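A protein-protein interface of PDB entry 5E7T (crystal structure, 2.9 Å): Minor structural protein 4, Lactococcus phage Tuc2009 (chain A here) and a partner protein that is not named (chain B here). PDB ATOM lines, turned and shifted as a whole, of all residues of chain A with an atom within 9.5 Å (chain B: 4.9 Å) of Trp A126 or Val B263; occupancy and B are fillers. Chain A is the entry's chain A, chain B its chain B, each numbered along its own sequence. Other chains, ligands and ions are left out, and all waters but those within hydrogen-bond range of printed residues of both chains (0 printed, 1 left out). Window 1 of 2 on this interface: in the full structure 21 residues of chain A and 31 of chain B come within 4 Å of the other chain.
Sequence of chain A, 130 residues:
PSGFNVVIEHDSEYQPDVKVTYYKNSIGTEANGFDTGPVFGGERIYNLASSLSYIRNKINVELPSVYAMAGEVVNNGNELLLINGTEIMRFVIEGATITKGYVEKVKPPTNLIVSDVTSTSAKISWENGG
Of chain B, only Tyr B231, Val B233, Ser B243, Leu B245, Leu B246, Ser B247, Phe B248 and Val B263 come within 4 Å of Trp A126. Val B263 touches just these residues of chain A: Pro A109 and Trp A126. Of chain A, only Ser A125, Trp A126, Glu A127 and Asn A128 come within 4 Å of Leu B246. Ser B264 touches just one residue of chain A: Pro A109. Ser B275 touches two residues of chain A. Of the printed residues of chain B, Lys A123 touches Ser B247 (3.6 Å) and Phe B248 (3.6 Å). Of the printed residues of chain B, Glu A127 touches Leu B246 (3.9 Å). Of the printed residues of chain A, Gln B265 touches Lys A107 (3.2 Å), Pro A109 (3.99 Å) and Asn A128 (3.3 Å). Printed residues of chain B within 4 Å of Pro A108: Asp B273. Asn A111 touches none of the printed residues of chain B. Ser A115 touches none of the printed residues of chain B. The nearest residue of chain A that does not touch Val B263 is Leu A112 (4.1 Å).
Of the 16 printed residues of chain B, 14 touch a printed residue of chain A. Hydrophobic or aromatic side chains of chain B within 4 Å of the printed part of chain A: Tyr B231, Val B233, Leu B246, Phe B248, Val B261 and Val B263. Printed residues of chain A that touch a printed residue of chain B: Lys A107, Pro A108, Pro A109, Leu A112, Lys A123, Ile A124, Ser A125, Trp A126, Glu A127 and Asn A128. Hydrophobic or aromatic side chains of chain A that line the printed part of chain B: Pro A108, Pro A109, Leu A112, Ile A124 and Trp A126.
OE1 of Gln B265 is in hydrogen-bond range of ND2 of Asn A128 (3.3 Å). O of Ile A124 sits at hydrogen-bond distance from N of Phe B248 (2.7 Å). O of Lys A107 lies close to OE1 of Gln B265 (3.2 Å). The backbone carbonyl oxygen (O) of Leu B246 lies within hydrogen-bond range of the backbone NH (N) of Trp A126, 3.0 Å away. ND2 of Asn A128 lies within hydrogen-bond range of OH of Tyr B231 (3.2 Å).
The backbone carbonyl oxygen of Ser B243 sits at hydrogen-bond distance from the backbone NH of Tyr B231 (3.0 Å). The backbone NH (N) of Ile A113 is in hydrogen-bond range of the backbone carbonyl oxygen (O) of Ser A125 (2.9 Å). NE2 of Gln B262 lies close to NZ of Lys B274. OG of Ser B243 lies within hydrogen-bond range of O of Leu B245 (3.1 Å). The side-chain carboxylate of Glu A127 sits close to the side-chain amide oxygen of Asn A111. The backbone carbonyl oxygen (O) of Ser A115 lies within hydrogen-bond range of the backbone NH (N) of Lys A123 (2.8 Å).
Among the printed residues, merely in contact across the chains: Pro A108 with Asp B273 (3.2 Å), Ile A124 with Ser B247 (3.3 Å), Trp A126 with Tyr B231 (3.3 Å), Pro A109 with Val B263 (3.3 Å), Ser A125 with Leu B246 (3.4 Å), Leu A112 with Ser B275 (3.4 Å), Pro A109 with Ser B275 (3.4 Å), Trp A126 with Ser B243 (3.5 Å), Trp A126 with Leu B245 (3.5 Å), Lys A123 with Phe B248 (3.6 Å), Asn A128 with Leu B246 (3.6 Å), Trp A126 with Ser B247 (3.6 Å), Lys A123 with Ser B247 (3.6 Å), Trp A126 with Phe B248 (3.7 Å), Leu A112 with Val B261 (3.8 Å), Trp A126 with Val B263 (3.8 Å), Ser A125 with Ser B247 (3.8 Å), Pro A109 with Ser B264 (3.8 Å), Ile A124 with Val B261 (3.9 Å), Glu A127 with Leu B246 (3.9 Å), Trp A126 with Val B233 (3.9 Å), Leu A112 with Gln B262 (3.97 Å) and Pro A109 with Gln B265 (3.99 Å).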
ATOM      1  N   LYS A 107      15.171  19.376  13.960  1.00  0.00           N
ATOM      2  CA  LYS A 107      13.994  18.546  13.786  1.00  0.00           C
ATOM      3  C   LYS A 107      14.025  17.692  12.496  1.00  0.00           C
ATOM      4  O   LYS A 107      14.465  18.148  11.435  1.00  0.00           O
ATOM      5  CB  LYS A 107      12.709  19.404  13.900  1.00  0.00           C
ATOM      6  CG  LYS A 107      12.405  19.837  15.346  1.00  0.00           C
ATOM      7  CD  LYS A 107      10.949  20.283  15.569  1.00  0.00           C
ATOM      8  CE  LYS A 107      10.600  20.473  17.033  1.00  0.00           C
ATOM      9  NZ  LYS A 107       9.261  21.102  17.207  1.00  0.00           N
ATOM     10  N   PRO A 108      13.525  16.443  12.599  1.00  0.00           N
ATOM     11  CA  PRO A 108      13.569  15.529  11.452  1.00  0.00           C
ATOM     12  C   PRO A 108      12.763  15.934  10.228  1.00  0.00           C
ATOM     13  O   PRO A 108      11.654  16.438  10.398  1.00  0.00           O
ATOM     14  CB  PRO A 108      13.037  14.209  12.018  1.00  0.00           C
ATOM     15  CG  PRO A 108      12.517  14.486  13.325  1.00  0.00           C
ATOM     16  CD  PRO A 108      13.049  15.761  13.818  1.00  0.00           C
ATOM     17  N   PRO A 109      13.275  15.643   9.000  1.00  0.00           N
ATOM     18  CA  PRO A 109      12.535  15.970   7.765  1.00  0.00           C
ATOM     19  C   PRO A 109      11.125  15.360   7.694  1.00  0.00           C
ATOM     20  O   PRO A 109      10.833  14.466   8.493  1.00  0.00           O
ATOM     21  CB  PRO A 109      13.466  15.464   6.666  1.00  0.00           C
ATOM     22  CG  PRO A 109      14.808  15.532   7.278  1.00  0.00           C
ATOM     23  CD  PRO A 109      14.591  15.069   8.675  1.00  0.00           C
ATOM     24  N   THR A 110      10.238  15.836   6.767  1.00  0.00           N
ATOM     25  CA  THR A 110       8.846  15.400   6.824  1.00  0.00           C
ATOM     26  C   THR A 110       8.198  14.764   5.586  1.00  0.00           C
ATOM     27  O   THR A 110       7.726  13.623   5.689  1.00  0.00           O
ATOM     28  CB  THR A 110       7.949  16.572   7.271  1.00  0.00           C
ATOM     29  OG1 THR A 110       8.512  17.157   8.435  1.00  0.00           O
ATOM     30  CG2 THR A 110       6.519  16.135   7.606  1.00  0.00           C
ATOM     31  N   ASN A 111       7.973  15.500   4.523  1.00  0.00           N
ATOM     32  CA  ASN A 111       7.164  14.879   3.494  1.00  0.00           C
ATOM     33  C   ASN A 111       8.010  14.134   2.507  1.00  0.00           C
ATOM     34  O   ASN A 111       8.322  14.647   1.428  1.00  0.00           O
ATOM     35  CB  ASN A 111       6.213  15.895   2.858  1.00  0.00           C
ATOM     36  CG  ASN A 111       5.196  16.424   3.860  1.00  0.00           C
ATOM     37  OD1 ASN A 111       5.435  17.392   4.605  1.00  0.00           O
ATOM     38  ND2 ASN A 111       4.055  15.756   3.940  1.00  0.00           N
ATOM     39  N   LEU A 112       8.405  12.912   2.889  1.00  0.00           N
ATOM     40  CA  LEU A 112       9.254  12.089   2.038  1.00  0.00           C
ATOM     41  C   LEU A 112       8.487  11.571   0.828  1.00  0.00           C
ATOM     42  O   LEU A 112       7.431  10.954   0.987  1.00  0.00           O
ATOM     43  CB  LEU A 112       9.907  10.954   2.840  1.00  0.00           C
ATOM     44  CG  LEU A 112      11.218  11.297   3.549  1.00  0.00           C
ATOM     45  CD1 LEU A 112      10.982  12.106   4.790  1.00  0.00           C
ATOM     46  CD2 LEU A 112      11.955  10.054   3.928  1.00  0.00           C
ATOM     47  N   ILE A 113       8.970  11.896  -0.380  1.00  0.00           N
ATOM     48  CA  ILE A 113       8.315  11.468  -1.617  1.00  0.00           C
ATOM     49  C   ILE A 113       9.333  10.811  -2.509  1.00  0.00           C
ATOM     50  O   ILE A 113      10.377  11.403  -2.788  1.00  0.00           O
ATOM     51  CB  ILE A 113       7.571  12.620  -2.393  1.00  0.00           C
ATOM     52  CG1 ILE A 113       6.621  13.481  -1.505  1.00  0.00           C
ATOM     53  CG2 ILE A 113       6.817  12.092  -3.624  1.00  0.00           C
ATOM     54  CD1 ILE A 113       5.290  12.788  -0.932  1.00  0.00           C
ATOM     55  N   VAL A 114       9.011   9.617  -3.006  1.00  0.00           N
ATOM     56  CA  VAL A 114       9.863   8.921  -3.972  1.00  0.00           C
ATOM     57  C   VAL A 114       9.300   9.172  -5.374  1.00  0.00           C
ATOM     58  O   VAL A 114       8.137   8.871  -5.646  1.00  0.00           O
ATOM     59  CB  VAL A 114      10.095   7.428  -3.656  1.00  0.00           C
ATOM     60  CG1 VAL A 114      11.235   7.266  -2.662  1.00  0.00           C
ATOM     61  CG2 VAL A 114       8.818   6.779  -3.118  1.00  0.00           C
ATOM     62  N   SER A 115      10.101   9.805  -6.225  1.00  0.00           N
ATOM     63  CA  SER A 115       9.747  10.181  -7.594  1.00  0.00           C
ATOM     64  C   SER A 115      10.832   9.695  -8.544  1.00  0.00           C
ATOM     65  O   SER A 115      11.874   9.229  -8.077  1.00  0.00           O
ATOM     66  CB  SER A 115       9.616  11.698  -7.694  1.00  0.00           C
ATOM     67  OG  SER A 115      10.663  12.369  -7.008  1.00  0.00           O
ATOM     68  N   ALA A 122      16.089   6.096  -8.083  1.00  0.00           N
ATOM     69  CA  ALA A 122      14.916   6.824  -7.569  1.00  0.00           C
ATOM     70  C   ALA A 122      15.367   8.151  -6.973  1.00  0.00           C
ATOM     71  O   ALA A 122      16.547   8.308  -6.653  1.00  0.00           O
ATOM     72  CB  ALA A 122      14.166   6.010  -6.527  1.00  0.00           C
ATOM     73  N   LYS A 123      14.444   9.114  -6.851  1.00  0.00           N
ATOM     74  CA  LYS A 123      14.737  10.432  -6.307  1.00  0.00           C
ATOM     75  C   LYS A 123      13.945  10.596  -5.036  1.00  0.00           C
ATOM     76  O   LYS A 123      12.729  10.374  -5.015  1.00  0.00           O
ATOM     77  CB  LYS A 123      14.401  11.544  -7.322  1.00  0.00           C
ATOM     78  CG  LYS A 123      14.953  12.923  -6.950  1.00  0.00           C
ATOM     79  CD  LYS A 123      14.927  13.913  -8.109  1.00  0.00           C
ATOM     80  CE  LYS A 123      13.737  14.841  -8.048  1.00  0.00           C
ATOM     81  NZ  LYS A 123      12.485  14.187  -8.521  1.00  0.00           N
ATOM     82  N   ILE A 124      14.639  10.937  -3.962  1.00  0.00           N
ATOM     83  CA  ILE A 124      14.002  11.137  -2.675  1.00  0.00           C
ATOM     84  C   ILE A 124      13.997  12.624  -2.415  1.00  0.00           C
ATOM     85  O   ILE A 124      15.034  13.265  -2.578  1.00  0.00           O
ATOM     86  CB  ILE A 124      14.629  10.276  -1.532  1.00  0.00           C
ATOM     87  CG1 ILE A 124      13.986  10.567  -0.153  1.00  0.00           C
ATOM     88  CG2 ILE A 124      16.154  10.406  -1.466  1.00  0.00           C
ATOM     89  CD1 ILE A 124      12.526  10.084   0.035  1.00  0.00           C
ATOM     90  N   SER A 125      12.817  13.179  -2.096  1.00  0.00           N
ATOM     91  CA  SER A 125      12.620  14.597  -1.811  1.00  0.00           C
ATOM     92  C   SER A 125      11.899  14.714  -0.474  1.00  0.00           C
ATOM     93  O   SER A 125      11.166  13.802  -0.088  1.00  0.00           O
ATOM     94  CB  SER A 125      11.804  15.247  -2.915  1.00  0.00           C
ATOM     95  OG  SER A 125      12.277  14.848  -4.191  1.00  0.00           O
ATOM     96  N   TRP A 126      12.130  15.800   0.256  1.00  0.00           N
ATOM     97  CA  TRP A 126      11.517  15.992   1.565  1.00  0.00           C
ATOM     98  C   TRP A 126      11.318  17.493   1.864  1.00  0.00           C
ATOM     99  O   TRP A 126      11.610  18.345   1.012  1.00  0.00           O
ATOM    100  CB  TRP A 126      12.371  15.289   2.656  1.00  0.00           C
ATOM    101  CG  TRP A 126      13.792  15.781   2.702  1.00  0.00           C
ATOM    102  CD1 TRP A 126      14.270  16.823   3.438  1.00  0.00           C
ATOM    103  CD2 TRP A 126      14.883  15.335   1.879  1.00  0.00           C
ATOM    104  NE1 TRP A 126      15.582  17.069   3.114  1.00  0.00           N
ATOM    105  CE2 TRP A 126      15.996  16.149   2.186  1.00  0.00           C
ATOM    106  CE3 TRP A 126      15.038  14.304   0.934  1.00  0.00           C
ATOM    107  CZ2 TRP A 126      17.251  15.955   1.597  1.00  0.00           C
ATOM    108  CZ3 TRP A 126      16.269  14.136   0.319  1.00  0.00           C
ATOM    109  CH2 TRP A 126      17.361  14.951   0.654  1.00  0.00           C
ATOM    110  N   GLU A 127      10.825  17.801   3.079  1.00  0.00           N
ATOM    111  CA  GLU A 127      10.598  19.159   3.580  1.00  0.00           C
ATOM    112  C   GLU A 127      11.196  19.271   5.013  1.00  0.00           C
ATOM    113  O   GLU A 127      11.006  18.350   5.804  1.00  0.00           O
ATOM    114  CB  GLU A 127       9.082  19.456   3.643  1.00  0.00           C
ATOM    115  CG  GLU A 127       8.310  19.316   2.340  1.00  0.00           C
ATOM    116  CD  GLU A 127       6.809  19.535   2.423  1.00  0.00           C
ATOM    117  OE1 GLU A 127       6.349  20.262   3.335  1.00  0.00           O
ATOM    118  OE2 GLU A 127       6.092  19.006   1.540  1.00  0.00           O
ATOM    119  N   ASN A 128      11.871  20.396   5.352  1.00  0.00           N
ATOM    120  CA  ASN A 128      12.467  20.639   6.679  1.00  0.00           C
ATOM    121  C   ASN A 128      11.397  20.657   7.796  1.00  0.00           C
ATOM    122  O   ASN A 128      10.316  21.227   7.601  1.00  0.00           O
ATOM    123  CB  ASN A 128      13.246  21.962   6.671  1.00  0.00           C
ATOM    124  CG  ASN A 128      14.034  22.260   7.932  1.00  0.00           C
ATOM    125  OD1 ASN A 128      13.493  22.696   8.962  1.00  0.00           O
ATOM    126  ND2 ASN A 128      15.348  22.109   7.852  1.00  0.00           N
ATOM    127  N   GLY A 129      11.723  20.054   8.946  1.00  0.00           N
ATOM    128  CA  GLY A 129      10.838  19.971  10.107  1.00  0.00           C
ATOM    129  C   GLY A 129      10.453  21.306  10.717  1.00  0.00           C
ATOM    130  O   GLY A 129      11.296  22.026  11.254  1.00  0.00           O
ATOM    131  N   TYR B 231      21.559  17.622   5.087  1.00  0.00           N
ATOM    132  CA  TYR B 231      20.773  16.383   5.256  1.00  0.00           C
ATOM    133  C   TYR B 231      21.573  15.099   5.029  1.00  0.00           C
ATOM    134  O   TYR B 231      22.530  15.105   4.269  1.00  0.00           O
ATOM    135  CB  TYR B 231      19.492  16.378   4.381  1.00  0.00           C
ATOM    136  CG  TYR B 231      18.639  17.619   4.527  1.00  0.00           C
ATOM    137  CD1 TYR B 231      17.710  17.733   5.558  1.00  0.00           C
ATOM    138  CD2 TYR B 231      18.807  18.706   3.677  1.00  0.00           C
ATOM    139  CE1 TYR B 231      16.954  18.892   5.723  1.00  0.00           C
ATOM    140  CE2 TYR B 231      18.076  19.877   3.847  1.00  0.00           C
ATOM    141  CZ  TYR B 231      17.151  19.970   4.874  1.00  0.00           C
ATOM    142  OH  TYR B 231      16.429  21.132   5.030  1.00  0.00           O
ATOM    143  N   ARG B 232      21.173  13.994   5.695  1.00  0.00           N
ATOM    144  CA  ARG B 232      21.821  12.684   5.570  1.00  0.00           C
ATOM    145  C   ARG B 232      20.782  11.683   5.163  1.00  0.00           C
ATOM    146  O   ARG B 232      19.756  11.570   5.832  1.00  0.00           O
ATOM    147  CB  ARG B 232      22.523  12.247   6.865  1.00  0.00           C
ATOM    148  CG  ARG B 232      23.795  11.505   6.544  1.00  0.00           C
ATOM    149  CD  ARG B 232      24.453  10.757   7.686  1.00  0.00           C
ATOM    150  NE  ARG B 232      25.005  11.569   8.787  1.00  0.00           N
ATOM    151  CZ  ARG B 232      25.936  12.514   8.686  1.00  0.00           C
ATOM    152  NH1 ARG B 232      26.361  12.918   7.494  1.00  0.00           N
ATOM    153  NH2 ARG B 232      26.402  13.106   9.770  1.00  0.00           N
ATOM    154  N   VAL B 233      21.024  10.990   4.037  1.00  0.00           N
ATOM    155  CA  VAL B 233      20.106  10.024   3.443  1.00  0.00           C
ATOM    156  C   VAL B 233      20.545   8.618   3.759  1.00  0.00           C
ATOM    157  O   VAL B 233      21.670   8.243   3.457  1.00  0.00           O
ATOM    158  CB  VAL B 233      19.912  10.296   1.939  1.00  0.00           C
ATOM    159  CG1 VAL B 233      19.086   9.200   1.269  1.00  0.00           C
ATOM    160  CG2 VAL B 233      19.277  11.671   1.721  1.00  0.00           C
ATOM    161  N   SER B 243      22.899  16.008   1.142  1.00  0.00           N
ATOM    162  CA  SER B 243      22.747  17.188   0.291  1.00  0.00           C
ATOM    163  C   SER B 243      22.516  18.474   1.065  1.00  0.00           C
ATOM    164  O   SER B 243      22.186  18.410   2.249  1.00  0.00           O
ATOM    165  CB  SER B 243      21.544  16.978  -0.631  1.00  0.00           C
ATOM    166  OG  SER B 243      20.426  16.503   0.106  1.00  0.00           O
ATOM    167  N   LEU B 245      20.409  20.630  -0.602  1.00  0.00           N
ATOM    168  CA  LEU B 245      19.050  20.730  -1.120  1.00  0.00           C
ATOM    169  C   LEU B 245      18.092  19.805  -0.405  1.00  0.00           C
ATOM    170  O   LEU B 245      18.536  18.965   0.364  1.00  0.00           O
ATOM    171  CB  LEU B 245      19.049  20.437  -2.626  1.00  0.00           C
ATOM    172  CG  LEU B 245      19.703  21.488  -3.497  1.00  0.00           C
ATOM    173  CD1 LEU B 245      19.931  20.958  -4.908  1.00  0.00           C
ATOM    174  CD2 LEU B 245      18.923  22.793  -3.449  1.00  0.00           C
ATOM    175  N   LEU B 246      16.779  19.950  -0.664  1.00  0.00           N
ATOM    176  CA  LEU B 246      15.706  19.140  -0.076  1.00  0.00           C
ATOM    177  C   LEU B 246      15.342  17.955  -0.997  1.00  0.00           C
ATOM    178  O   LEU B 246      14.191  17.513  -1.009  1.00  0.00           O
ATOM    179  CB  LEU B 246      14.458  20.019   0.168  1.00  0.00           C
ATOM    180  CG  LEU B 246      14.545  21.093   1.244  1.00  0.00           C
ATOM    181  CD1 LEU B 246      13.651  22.244   0.903  1.00  0.00           C
ATOM    182  CD2 LEU B 246      14.141  20.555   2.589  1.00  0.00           C
ATOM    183  N   SER B 247      16.324  17.446  -1.759  1.00  0.00           N
ATOM    184  CA  SER B 247      16.177  16.346  -2.721  1.00  0.00           C
ATOM    185  C   SER B 247      17.519  15.614  -2.877  1.00  0.00           C
ATOM    186  O   SER B 247      18.577  16.238  -2.747  1.00  0.00           O
ATOM    187  CB  SER B 247      15.726  16.899  -4.075  1.00  0.00           C
ATOM    188  OG  SER B 247      15.790  15.959  -5.134  1.00  0.00           O
ATOM    189  N   PHE B 248      17.482  14.304  -3.159  1.00  0.00           N
ATOM    190  CA  PHE B 248      18.680  13.480  -3.335  1.00  0.00           C
ATOM    191  C   PHE B 248      18.390  12.334  -4.284  1.00  0.00           C
ATOM    192  O   PHE B 248      17.314  11.735  -4.204  1.00  0.00           O
ATOM    193  CB  PHE B 248      19.161  12.932  -1.982  1.00  0.00           C
ATOM    194  CG  PHE B 248      20.386  12.051  -2.046  1.00  0.00           C
ATOM    195  CD1 PHE B 248      21.659  12.604  -2.048  1.00  0.00           C
ATOM    196  CD2 PHE B 248      20.267  10.667  -2.058  1.00  0.00           C
ATOM    197  CE1 PHE B 248      22.787  11.787  -2.064  1.00  0.00           C
ATOM    198  CE2 PHE B 248      21.399   9.848  -2.080  1.00  0.00           C
ATOM    199  CZ  PHE B 248      22.647  10.412  -2.061  1.00  0.00           C
ATOM    200  N   VAL B 261      13.859   4.245   2.738  1.00  0.00           N
ATOM    201  CA  VAL B 261      14.666   5.446   2.850  1.00  0.00           C
ATOM    202  C   VAL B 261      14.073   6.319   3.942  1.00  0.00           C
ATOM    203  O   VAL B 261      12.852   6.396   4.119  1.00  0.00           O
ATOM    204  CB  VAL B 261      14.873   6.181   1.475  1.00  0.00           C
ATOM    205  CG1 VAL B 261      13.561   6.393   0.741  1.00  0.00           C
ATOM    206  CG2 VAL B 261      15.639   7.501   1.605  1.00  0.00           C
ATOM    207  N   GLN B 262      14.965   6.904   4.717  1.00  0.00           N
ATOM    208  CA  GLN B 262      14.675   7.840   5.788  1.00  0.00           C
ATOM    209  C   GLN B 262      15.804   8.877   5.732  1.00  0.00           C
ATOM    210  O   GLN B 262      16.907   8.545   5.278  1.00  0.00           O
ATOM    211  CB  GLN B 262      14.526   7.136   7.151  1.00  0.00           C
ATOM    212  CG  GLN B 262      15.626   6.152   7.487  1.00  0.00           C
ATOM    213  CD  GLN B 262      15.415   5.373   8.749  1.00  0.00           C
ATOM    214  OE1 GLN B 262      14.408   5.532   9.467  1.00  0.00           O
ATOM    215  NE2 GLN B 262      16.403   4.534   9.072  1.00  0.00           N
ATOM    216  N   VAL B 263      15.489  10.150   6.063  1.00  0.00           N
ATOM    217  CA  VAL B 263      16.440  11.272   6.017  1.00  0.00           C
ATOM    218  C   VAL B 263      16.529  11.904   7.398  1.00  0.00           C
ATOM    219  O   VAL B 263      15.540  11.921   8.129  1.00  0.00           O
ATOM    220  CB  VAL B 263      16.027  12.337   4.957  1.00  0.00           C
ATOM    221  CG1 VAL B 263      17.057  13.466   4.838  1.00  0.00           C
ATOM    222  CG2 VAL B 263      15.737  11.704   3.592  1.00  0.00           C
ATOM    223  N   SER B 264      17.706  12.435   7.744  1.00  0.00           N
ATOM    224  CA  SER B 264      17.919  13.197   8.972  1.00  0.00           C
ATOM    225  C   SER B 264      18.482  14.582   8.581  1.00  0.00           C
ATOM    226  O   SER B 264      18.904  14.761   7.432  1.00  0.00           O
ATOM    227  CB  SER B 264      18.868  12.460   9.900  1.00  0.00           C
ATOM    228  OG  SER B 264      20.196  12.622   9.449  1.00  0.00           O
ATOM    229  N   GLN B 265      18.464  15.557   9.508  1.00  0.00           N
ATOM    230  CA  GLN B 265      19.003  16.895   9.266  1.00  0.00           C
ATOM    231  C   GLN B 265      20.286  17.056  10.058  1.00  0.00           C
ATOM    232  O   GLN B 265      20.351  16.655  11.228  1.00  0.00           O
ATOM    233  CB  GLN B 265      18.003  17.987   9.672  1.00  0.00           C
ATOM    234  CG  GLN B 265      18.464  19.404   9.336  1.00  0.00           C
ATOM    235  CD  GLN B 265      17.729  20.505  10.058  1.00  0.00           C
ATOM    236  OE1 GLN B 265      16.545  20.393  10.376  1.00  0.00           O
ATOM    237  NE2 GLN B 265      18.411  21.624  10.281  1.00  0.00           N
ATOM    238  N   ASP B 273      16.784  13.310  14.816  1.00  0.00           N
ATOM    239  CA  ASP B 273      16.359  11.917  14.816  1.00  0.00           C
ATOM    240  C   ASP B 273      16.008  11.621  13.364  1.00  0.00           C
ATOM    241  O   ASP B 273      15.741  12.557  12.615  1.00  0.00           O
ATOM    242  CB  ASP B 273      15.135  11.719  15.717  1.00  0.00           C
ATOM    243  CG  ASP B 273      15.412  11.775  17.216  1.00  0.00           C
ATOM    244  OD1 ASP B 273      16.581  11.538  17.619  1.00  0.00           O
ATOM    245  OD2 ASP B 273      14.449  12.024  17.995  1.00  0.00           O
ATOM    246  N   LYS B 274      16.075  10.350  12.928  1.00  0.00           N
ATOM    247  CA  LYS B 274      15.773  10.047  11.526  1.00  0.00           C
ATOM    248  C   LYS B 274      14.276  10.247  11.249  1.00  0.00           C
ATOM    249  O   LYS B 274      13.451  10.074  12.153  1.00  0.00           O
ATOM    250  CB  LYS B 274      16.257   8.638  11.146  1.00  0.00           C
ATOM    251  CG  LYS B 274      17.770   8.450  11.248  1.00  0.00           C
ATOM    252  CD  LYS B 274      18.207   7.081  10.728  1.00  0.00           C
ATOM    253  CE  LYS B 274      18.828   6.152  11.755  1.00  0.00           C
ATOM    254  NZ  LYS B 274      18.881   4.744  11.249  1.00  0.00           N
ATOM    255  N   SER B 275      13.927  10.649  10.025  1.00  0.00           N
ATOM    256  CA  SER B 275      12.530  10.826   9.606  1.00  0.00           C
ATOM    257  C   SER B 275      11.792   9.487   9.564  1.00  0.00           C
ATOM    258  O   SER B 275      12.406   8.417   9.667  1.00  0.00           O
ATOM    259  CB  SER B 275      12.461  11.443   8.211  1.00  0.00           C
ATOM    260  OG  SER B 275      12.698  10.444   7.232  1.00  0.00           O
